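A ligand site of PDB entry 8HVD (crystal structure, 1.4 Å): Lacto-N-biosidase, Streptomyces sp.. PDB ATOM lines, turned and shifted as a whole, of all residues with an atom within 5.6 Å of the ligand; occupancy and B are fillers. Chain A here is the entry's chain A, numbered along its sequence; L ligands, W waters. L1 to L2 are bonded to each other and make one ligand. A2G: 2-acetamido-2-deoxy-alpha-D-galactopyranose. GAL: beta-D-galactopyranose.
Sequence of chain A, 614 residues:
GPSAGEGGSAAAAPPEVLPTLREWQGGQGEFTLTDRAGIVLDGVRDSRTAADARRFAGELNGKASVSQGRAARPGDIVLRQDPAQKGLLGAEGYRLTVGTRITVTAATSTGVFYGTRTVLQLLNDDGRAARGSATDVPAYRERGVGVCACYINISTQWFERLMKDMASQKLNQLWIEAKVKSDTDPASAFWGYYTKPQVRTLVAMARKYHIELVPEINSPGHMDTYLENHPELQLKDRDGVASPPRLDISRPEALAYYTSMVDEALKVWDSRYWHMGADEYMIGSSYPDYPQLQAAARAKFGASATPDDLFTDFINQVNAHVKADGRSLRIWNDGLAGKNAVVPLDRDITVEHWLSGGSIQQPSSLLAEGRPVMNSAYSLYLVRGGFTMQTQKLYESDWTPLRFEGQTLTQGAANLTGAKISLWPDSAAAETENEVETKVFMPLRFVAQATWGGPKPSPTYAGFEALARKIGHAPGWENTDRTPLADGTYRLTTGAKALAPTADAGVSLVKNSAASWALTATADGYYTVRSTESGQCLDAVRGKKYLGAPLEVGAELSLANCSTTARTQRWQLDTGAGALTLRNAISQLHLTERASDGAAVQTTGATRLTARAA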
ATOM      1  N   CYS A 148      -6.059  23.039   1.779  1.00  0.00           N
ATOM      2  CA  CYS A 148      -5.485  22.039   2.697  1.00  0.00           C
ATOM      3  C   CYS A 148      -6.643  21.280   3.373  1.00  0.00           C
ATOM      4  O   CYS A 148      -7.254  21.795   4.344  1.00  0.00           O
ATOM      5  CB  CYS A 148      -4.599  22.709   3.705  1.00  0.00           C
ATOM      6  SG  CYS A 148      -3.751  21.590   4.872  1.00  0.00           S
ATOM      7  N   CYS A 150      -6.792  18.705   5.325  1.00  0.00           N
ATOM      8  CA  CYS A 150      -5.991  17.891   6.219  1.00  0.00           C
ATOM      9  C   CYS A 150      -6.541  17.911   7.611  1.00  0.00           C
ATOM     10  O   CYS A 150      -7.054  18.952   8.046  1.00  0.00           O
ATOM     11  CB  CYS A 150      -4.568  18.360   6.403  1.00  0.00           C
ATOM     12  SG  CYS A 150      -3.686  18.343   4.837  1.00  0.00           S
ATOM     13  N   TYR A 151      -6.393  16.750   8.280  1.00  0.00           N
ATOM     14  CA  TYR A 151      -6.998  16.471   9.583  1.00  0.00           C
ATOM     15  C   TYR A 151      -8.510  16.361   9.438  1.00  0.00           C
ATOM     16  O   TYR A 151      -9.079  15.267   9.505  1.00  0.00           O
ATOM     17  CB  TYR A 151      -6.547  17.473  10.673  1.00  0.00           C
ATOM     18  CG  TYR A 151      -5.065  17.599  10.868  1.00  0.00           C
ATOM     19  CD1 TYR A 151      -4.416  16.787  11.770  1.00  0.00           C
ATOM     20  CD2 TYR A 151      -4.315  18.538  10.183  1.00  0.00           C
ATOM     21  CE1 TYR A 151      -3.054  16.917  12.029  1.00  0.00           C
ATOM     22  CE2 TYR A 151      -2.949  18.689  10.404  1.00  0.00           C
ATOM     23  CZ  TYR A 151      -2.327  17.872  11.320  1.00  0.00           C
ATOM     24  OH  TYR A 151      -0.958  18.045  11.470  1.00  0.00           O
ATOM     25  N   GLU A 177      -3.748  19.457  -0.362  1.00  0.00           N
ATOM     26  CA  GLU A 177      -3.040  18.638   0.609  1.00  0.00           C
ATOM     27  C   GLU A 177      -4.092  17.802   1.293  1.00  0.00           C
ATOM     28  O   GLU A 177      -5.015  18.368   1.865  1.00  0.00           O
ATOM     29  CB  GLU A 177      -2.251  19.488   1.606  1.00  0.00           C
ATOM     30  CG  GLU A 177      -1.359  18.689   2.542  1.00  0.00           C
ATOM     31  CD  GLU A 177      -0.715  19.515   3.645  1.00  0.00           C
ATOM     32  OE1 GLU A 177      -0.780  20.786   3.575  1.00  0.00           O
ATOM     33  OE2 GLU A 177      -0.152  18.888   4.562  1.00  0.00           O
ATOM     34  N   GLU A 216      -0.430  17.153  -2.502  1.00  0.00           N
ATOM     35  CA  GLU A 216       0.718  17.217  -1.606  1.00  0.00           C
ATOM     36  C   GLU A 216       0.581  16.209  -0.470  1.00  0.00           C
ATOM     37  O   GLU A 216      -0.484  16.056   0.167  1.00  0.00           O
ATOM     38  CB  GLU A 216       0.838  18.607  -0.976  1.00  0.00           C
ATOM     39  CG  GLU A 216       2.014  18.697  -0.012  1.00  0.00           C
ATOM     40  CD  GLU A 216       2.139  20.048   0.665  1.00  0.00           C
ATOM     41  OE1 GLU A 216       1.976  21.088   0.047  1.00  0.00           O
ATOM     42  OE2 GLU A 216       2.422  20.005   1.915  1.00  0.00           O
ATOM     43  N   ASN A 218       2.878  16.484   2.830  1.00  0.00           N
ATOM     44  CA  ASN A 218       3.946  17.282   3.426  1.00  0.00           C
ATOM     45  C   ASN A 218       4.969  16.360   4.049  1.00  0.00           C
ATOM     46  O   ASN A 218       4.596  15.305   4.589  1.00  0.00           O
ATOM     47  CB  ASN A 218       3.374  18.312   4.396  1.00  0.00           C
ATOM     48  CG  ASN A 218       4.279  19.505   4.595  1.00  0.00           C
ATOM     49  OD1 ASN A 218       5.381  19.542   4.039  1.00  0.00           O
ATOM     50  ND2 ASN A 218       3.773  20.516   5.274  1.00  0.00           N
ATOM     51  N   HIS A 222       5.764  17.720   9.466  1.00  0.00           N
ATOM     52  CA  HIS A 222       4.335  17.839   9.309  1.00  0.00           C
ATOM     53  C   HIS A 222       3.696  16.529   8.891  1.00  0.00           C
ATOM     54  O   HIS A 222       2.625  16.510   8.301  1.00  0.00           O
ATOM     55  CB  HIS A 222       3.962  18.975   8.329  1.00  0.00           C
ATOM     56  CG  HIS A 222       4.414  20.307   8.704  1.00  0.00           C
ATOM     57  ND1 HIS A 222       5.507  20.899   8.128  1.00  0.00           N
ATOM     58  CD2 HIS A 222       3.899  21.165   9.589  1.00  0.00           C
ATOM     59  CE1 HIS A 222       5.695  22.105   8.704  1.00  0.00           C
ATOM     60  NE2 HIS A 222       4.642  22.314   9.540  1.00  0.00           N
ATOM     61  N   ASP A 279       8.665  22.178   3.928  1.00  0.00           N
ATOM     62  CA  ASP A 279       8.871  23.327   4.805  1.00  0.00           C
ATOM     63  C   ASP A 279      10.144  23.102   5.620  1.00  0.00           C
ATOM     64  O   ASP A 279      10.616  21.987   5.757  1.00  0.00           O
ATOM     65  CB  ASP A 279       7.688  23.549   5.731  1.00  0.00           C
ATOM     66  CG  ASP A 279       6.410  23.853   4.980  1.00  0.00           C
ATOM     67  OD1 ASP A 279       6.391  24.907   4.291  1.00  0.00           O
ATOM     68  OD2 ASP A 279       5.392  23.143   5.164  1.00  0.00           O
ATOM     69  N   TRP A 332       7.429  24.047  -1.072  1.00  0.00           N
ATOM     70  CA  TRP A 332       7.408  25.382  -0.491  1.00  0.00           C
ATOM     71  C   TRP A 332       8.818  25.943  -0.394  1.00  0.00           C
ATOM     72  O   TRP A 332       9.799  25.228  -0.534  1.00  0.00           O
ATOM     73  CB  TRP A 332       6.744  25.347   0.896  1.00  0.00           C
ATOM     74  CG  TRP A 332       5.324  24.875   0.935  1.00  0.00           C
ATOM     75  CD1 TRP A 332       4.836  23.784   1.586  1.00  0.00           C
ATOM     76  CD2 TRP A 332       4.205  25.474   0.281  1.00  0.00           C
ATOM     77  NE1 TRP A 332       3.481  23.716   1.445  1.00  0.00           N
ATOM     78  CE2 TRP A 332       3.069  24.734   0.639  1.00  0.00           C
ATOM     79  CE3 TRP A 332       4.033  26.638  -0.498  1.00  0.00           C
ATOM     80  CZ2 TRP A 332       1.802  25.106   0.227  1.00  0.00           C
ATOM     81  CZ3 TRP A 332       2.775  26.974  -0.929  1.00  0.00           C
ATOM     82  CH2 TRP A 332       1.680  26.205  -0.592  1.00  0.00           C
ATOM     83  N   ASP A 334      10.259  27.847   2.297  1.00  0.00           N
ATOM     84  CA  ASP A 334      10.760  28.368   3.579  1.00  0.00           C
ATOM     85  C   ASP A 334      11.932  27.581   4.163  1.00  0.00           C
ATOM     86  O   ASP A 334      12.572  28.077   5.072  1.00  0.00           O
ATOM     87  CB  ASP A 334       9.591  28.448   4.563  1.00  0.00           C
ATOM     88  CG  ASP A 334       8.922  27.103   4.830  1.00  0.00           C
ATOM     89  OD1 ASP A 334       8.273  26.589   3.889  1.00  0.00           O
ATOM     90  OD2 ASP A 334       9.082  26.554   5.936  1.00  0.00           O
ATOM     91  N   TRP A 354       5.862  31.488  -0.140  1.00  0.00           N
ATOM     92  CA  TRP A 354       4.841  31.990   0.756  1.00  0.00           C
ATOM     93  C   TRP A 354       5.396  32.842   1.895  1.00  0.00           C
ATOM     94  O   TRP A 354       4.599  33.581   2.487  1.00  0.00           O
ATOM     95  CB  TRP A 354       3.967  30.862   1.359  1.00  0.00           C
ATOM     96  CG  TRP A 354       4.707  29.955   2.280  1.00  0.00           C
ATOM     97  CD1 TRP A 354       5.562  28.940   1.956  1.00  0.00           C
ATOM     98  CD2 TRP A 354       4.697  30.030   3.706  1.00  0.00           C
ATOM     99  NE1 TRP A 354       6.073  28.365   3.093  1.00  0.00           N
ATOM    100  CE2 TRP A 354       5.567  29.016   4.175  1.00  0.00           C
ATOM    101  CE3 TRP A 354       4.030  30.825   4.663  1.00  0.00           C
ATOM    102  CZ2 TRP A 354       5.813  28.808   5.537  1.00  0.00           C
ATOM    103  CZ3 TRP A 354       4.265  30.588   6.029  1.00  0.00           C
ATOM    104  CH2 TRP A 354       5.171  29.621   6.454  1.00  0.00           C
ATOM    105  N   TYR A 378       1.690  34.410   1.806  1.00  0.00           N
ATOM    106  CA  TYR A 378       0.918  34.427   3.048  1.00  0.00           C
ATOM    107  C   TYR A 378      -0.230  35.415   2.957  1.00  0.00           C
ATOM    108  O   TYR A 378      -1.307  35.165   3.462  1.00  0.00           O
ATOM    109  CB  TYR A 378       1.851  34.753   4.217  1.00  0.00           C
ATOM    110  CG  TYR A 378       1.244  34.463   5.555  1.00  0.00           C
ATOM    111  CD1 TYR A 378       0.259  35.232   6.133  1.00  0.00           C
ATOM    112  CD2 TYR A 378       1.673  33.359   6.237  1.00  0.00           C
ATOM    113  CE1 TYR A 378      -0.259  34.861   7.384  1.00  0.00           C
ATOM    114  CE2 TYR A 378       1.207  32.988   7.463  1.00  0.00           C
ATOM    115  CZ  TYR A 378       0.200  33.732   8.018  1.00  0.00           C
ATOM    116  OH  TYR A 378      -0.118  33.226   9.284  1.00  0.00           O
ATOM    117  N   TYR A 381      -3.706  34.182   2.013  1.00  0.00           N
ATOM    118  CA  TYR A 381      -4.254  33.089   2.797  1.00  0.00           C
ATOM    119  C   TYR A 381      -5.666  33.378   3.328  1.00  0.00           C
ATOM    120  O   TYR A 381      -6.002  34.510   3.683  1.00  0.00           O
ATOM    121  CB  TYR A 381      -3.351  32.817   4.006  1.00  0.00           C
ATOM    122  CG  TYR A 381      -2.091  32.038   3.779  1.00  0.00           C
ATOM    123  CD1 TYR A 381      -1.606  31.741   2.498  1.00  0.00           C
ATOM    124  CD2 TYR A 381      -1.303  31.643   4.847  1.00  0.00           C
ATOM    125  CE1 TYR A 381      -0.470  30.993   2.315  1.00  0.00           C
ATOM    126  CE2 TYR A 381      -0.188  30.866   4.665  1.00  0.00           C
ATOM    127  CZ  TYR A 381       0.269  30.534   3.405  1.00  0.00           C
ATOM    128  OH  TYR A 381       1.381  29.777   3.260  1.00  0.00           O
ATOM    129  N   VAL A 383      -7.491  31.318   6.643  1.00  0.00           N
ATOM    130  CA  VAL A 383      -7.212  30.362   7.691  1.00  0.00           C
ATOM    131  C   VAL A 383      -8.382  30.242   8.666  1.00  0.00           C
ATOM    132  O   VAL A 383      -8.838  31.256   9.208  1.00  0.00           O
ATOM    133  CB  VAL A 383      -5.964  30.790   8.463  1.00  0.00           C
ATOM    134  CG1 VAL A 383      -5.548  29.778   9.490  1.00  0.00           C
ATOM    135  CG2 VAL A 383      -4.785  31.107   7.534  1.00  0.00           C
ATOM    136  N   TRP A 424      -6.518  27.186   4.584  1.00  0.00           N
ATOM    137  CA  TRP A 424      -5.914  26.384   5.633  1.00  0.00           C
ATOM    138  C   TRP A 424      -6.907  26.161   6.771  1.00  0.00           C
ATOM    139  O   TRP A 424      -7.709  27.033   7.079  1.00  0.00           O
ATOM    140  CB  TRP A 424      -4.687  27.074   6.211  1.00  0.00           C
ATOM    141  CG  TRP A 424      -3.670  27.422   5.200  1.00  0.00           C
ATOM    142  CD1 TRP A 424      -3.502  28.620   4.597  1.00  0.00           C
ATOM    143  CD2 TRP A 424      -2.659  26.541   4.676  1.00  0.00           C
ATOM    144  NE1 TRP A 424      -2.409  28.560   3.788  1.00  0.00           N
ATOM    145  CE2 TRP A 424      -1.887  27.298   3.775  1.00  0.00           C
ATOM    146  CE3 TRP A 424      -2.334  25.202   4.910  1.00  0.00           C
ATOM    147  CZ2 TRP A 424      -0.791  26.724   3.139  1.00  0.00           C
ATOM    148  CZ3 TRP A 424      -1.271  24.634   4.248  1.00  0.00           C
ATOM    149  CH2 TRP A 424      -0.506  25.396   3.366  1.00  0.00           C
ATOM    150  N   PRO A 425      -6.896  24.998   7.434  1.00  0.00           N
ATOM    151  CA  PRO A 425      -7.850  24.681   8.503  1.00  0.00           C
ATOM    152  C   PRO A 425      -7.323  24.769   9.920  1.00  0.00           C
ATOM    153  O   PRO A 425      -7.900  24.139  10.802  1.00  0.00           O
ATOM    154  CB  PRO A 425      -8.134  23.206   8.178  1.00  0.00           C
ATOM    155  CG  PRO A 425      -6.785  22.691   7.832  1.00  0.00           C
ATOM    156  CD  PRO A 425      -6.171  23.801   7.013  1.00  0.00           C
ATOM    157  N   ASP A 426      -6.312  25.619  10.147  1.00  0.00           N
ATOM    158  CA  ASP A 426      -5.585  25.580  11.410  1.00  0.00           C
ATOM    159  C   ASP A 426      -6.450  25.409  12.660  1.00  0.00           C
ATOM    160  O   ASP A 426      -6.176  24.511  13.456  1.00  0.00           O
ATOM    161  CB  ASP A 426      -4.766  26.870  11.604  1.00  0.00           C
ATOM    162  CG  ASP A 426      -3.551  27.048  10.706  1.00  0.00           C
ATOM    163  OD1 ASP A 426      -3.443  26.343   9.666  1.00  0.00           O
ATOM    164  OD2 ASP A 426      -2.770  28.007  10.970  1.00  0.00           O
ATOM    165  N   LEU A 547      -6.446  19.634  15.683  1.00  0.00           N
ATOM    166  CA  LEU A 547      -6.728  21.025  15.384  1.00  0.00           C
ATOM    167  C   LEU A 547      -8.015  21.507  16.052  1.00  0.00           C
ATOM    168  O   LEU A 547      -8.698  22.384  15.583  1.00  0.00           O
ATOM    169  CB  LEU A 547      -6.859  21.233  13.856  1.00  0.00           C
ATOM    170  CG  LEU A 547      -5.700  20.790  12.984  1.00  0.00           C
ATOM    171  CD1 LEU A 547      -5.932  21.210  11.566  1.00  0.00           C
ATOM    172  CD2 LEU A 547      -4.400  21.362  13.491  1.00  0.00           C
HETATM  173  O5  A2G L   1       0.566  28.990   7.578  1.00  0.00           O
HETATM  174  C1  A2G L   1       1.812  28.467   7.139  1.00  0.00           C
HETATM  175  O1  A2G L   1       1.879  28.311   5.735  1.00  0.00           O
HETATM  176  C2  A2G L   1       1.987  27.118   7.806  1.00  0.00           C
HETATM  177  N2  A2G L   1       3.267  26.543   7.451  1.00  0.00           N
HETATM  178  C3  A2G L   1       0.875  26.201   7.338  1.00  0.00           C
HETATM  179  O3  A2G L   1       1.121  24.924   7.867  1.00  0.00           O
HETATM  180  C4  A2G L   1      -0.466  26.769   7.771  1.00  0.00           C
HETATM  181  O4  A2G L   1      -0.540  26.727   9.207  1.00  0.00           O
HETATM  182  C5  A2G L   1      -0.576  28.184   7.210  1.00  0.00           C
HETATM  183  C6  A2G L   1      -1.765  28.999   7.674  1.00  0.00           C
HETATM  184  O6  A2G L   1      -1.643  29.469   9.059  1.00  0.00           O
HETATM  185  C7  A2G L   1       4.285  26.653   8.294  1.00  0.00           C
HETATM  186  O7  A2G L   1       4.233  27.376   9.295  1.00  0.00           O
HETATM  187  C8  A2G L   1       5.546  25.948   7.913  1.00  0.00           C
HETATM  188  C1  GAL L   2       0.246  23.833   7.351  1.00  0.00           C
HETATM  189  C2  GAL L   2       1.084  22.620   7.056  1.00  0.00           C
HETATM  190  C3  GAL L   2       0.202  21.486   6.649  1.00  0.00           C
HETATM  191  C4  GAL L   2      -0.910  21.272   7.674  1.00  0.00           C
HETATM  192  C5  GAL L   2      -1.644  22.573   7.938  1.00  0.00           C
HETATM  193  C6  GAL L   2      -2.689  22.449   9.006  1.00  0.00           C
HETATM  194  O2  GAL L   2       1.975  22.862   5.962  1.00  0.00           O
HETATM  195  O3  GAL L   2       0.988  20.326   6.464  1.00  0.00           O
HETATM  196  O4  GAL L   2      -0.369  20.728   8.901  1.00  0.00           O
HETATM  197  O5  GAL L   2      -0.701  23.581   8.393  1.00  0.00           O
HETATM  198  O6  GAL L   2      -3.576  23.601   8.978  1.00  0.00           O
HETATM  199  O   HOH W   1       5.905  26.707  11.366  1.00  0.00           O
HETATM  200  O   HOH W   2       1.238  25.162  10.891  1.00  0.00           O
HETATM  201  O   HOH W   3       3.873  24.583  10.797  1.00  0.00           O
HETATM  202  O   HOH W   4       0.783  30.643  10.020  1.00  0.00           O
HETATM  203  O   HOH W   5       3.558  30.257   9.591  1.00  0.00           O
HETATM  204  O   HOH W   6       0.298  18.020   8.985  1.00  0.00           O
HETATM  205  O   HOH W   7       2.868  27.038   3.121  1.00  0.00           O
HETATM  206  O   HOH W   8       1.532  22.148   3.251  1.00  0.00           O
HETATM  207  O   HOH W   9       3.303  25.080   4.973  1.00  0.00           O
HETATM  208  O   HOH W  10       1.073  22.291  10.727  1.00  0.00           O
HETATM  209  O   HOH W  11      -2.336  32.065   9.885  1.00  0.00           O
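The side-chain carboxylate (OE2) of Glu 177 sits at hydrogen-bond distance from an oxygen (O3) of GAL L2, 2.6 Å away. O6 of A2G L1 lies within hydrogen-bond range of OD2 of Asp 426 (2.7 Å). O1 of A2G L1 lies within hydrogen-bond range of OH of Tyr 381, 2.9 Å away. The side-chain amide nitrogen of Asn 218 sits at hydrogen-bond distance from an oxygen (O2) of GAL L2 (3.0 Å).
Water W9 lies within hydrogen-bond range of an oxygen (O2) of GAL L2 (2.8 Å) and the side-chain carboxylate of Asp 279 (2.9 Å). Water W6 lies within hydrogen-bond range of the side-chain hydroxyl (OH) of Tyr 151 (2.8 Å), an oxygen (O4) of GAL L2 (2.8 Å) and the backbone carbonyl oxygen (O) of His 222 (2.9 Å). Water W11 lies within hydrogen-bond range of OH of Tyr 378 (2.6 Å) and O6 of A2G L1 (2.8 Å). Water W4 lies within hydrogen-bond range of the side-chain hydroxyl of Tyr 378 (2.8 Å) and an oxygen (O6) of A2G L1 (2.9 Å). Water W7 lies within hydrogen-bond range of O1 of A2G L1 (3.1 Å), OH of Tyr 381 (3.1 Å) and NE1 of Trp 354 (3.5 Å). Water W3 bridges NE2 of His 222 (2.7 Å) and O7 of A2G L1 (3.2 Å).
The side-chain sulfur (SG) of Cys 148 sits at hydrogen-bond distance from the side-chain carboxylate (OE1) of Glu 177 (3.3 Å). The backbone carbonyl oxygen (O) of Glu 177 sits at hydrogen-bond distance from the side-chain sulfur (SG) of Cys 150. The side-chain amide nitrogen (ND2) of Asn 218 sits at hydrogen-bond distance from the side-chain carboxylate (OD2) of Asp 279 (3.1 Å). The side-chain amide nitrogen of Asn 218 sits at hydrogen-bond distance from a ring nitrogen (ND1) of His 222, at 3.4 Å. O of Trp 354 lies within hydrogen-bond range of N of Tyr 378, 3.1 Å away. The indole nitrogen (NE1) of Trp 354 lies within hydrogen-bond range of the side-chain carboxylate (OD1) of Asp 334 (2.9 Å). OD1 of Asp 334 lies close to OD1 of Asp 279 (2.6 Å). The side-chain sulfur (SG) of Cys 148 is in hydrogen-bond range of the side-chain sulfur (SG) of Cys 150 (3.2 Å).
Residues that only touch the ligand: Pro 425, Trp 354, Trp 424, Asp 279, Tyr 151, Val 383, His 222 and Cys 148. 12 residues have an atom within 4 Å of the ligand: Cys 148, Tyr 151, Glu 177, Asn 218, His 222, Asp 279, Trp 354, Tyr 381, Val 383, Trp 424, Pro 425 and Asp 426. Along chain A the residues within 4 Å of the ligand span positions 148 to 426. The nearest printed residue that does not touch the ligand is Tyr 378 (4.1 Å).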
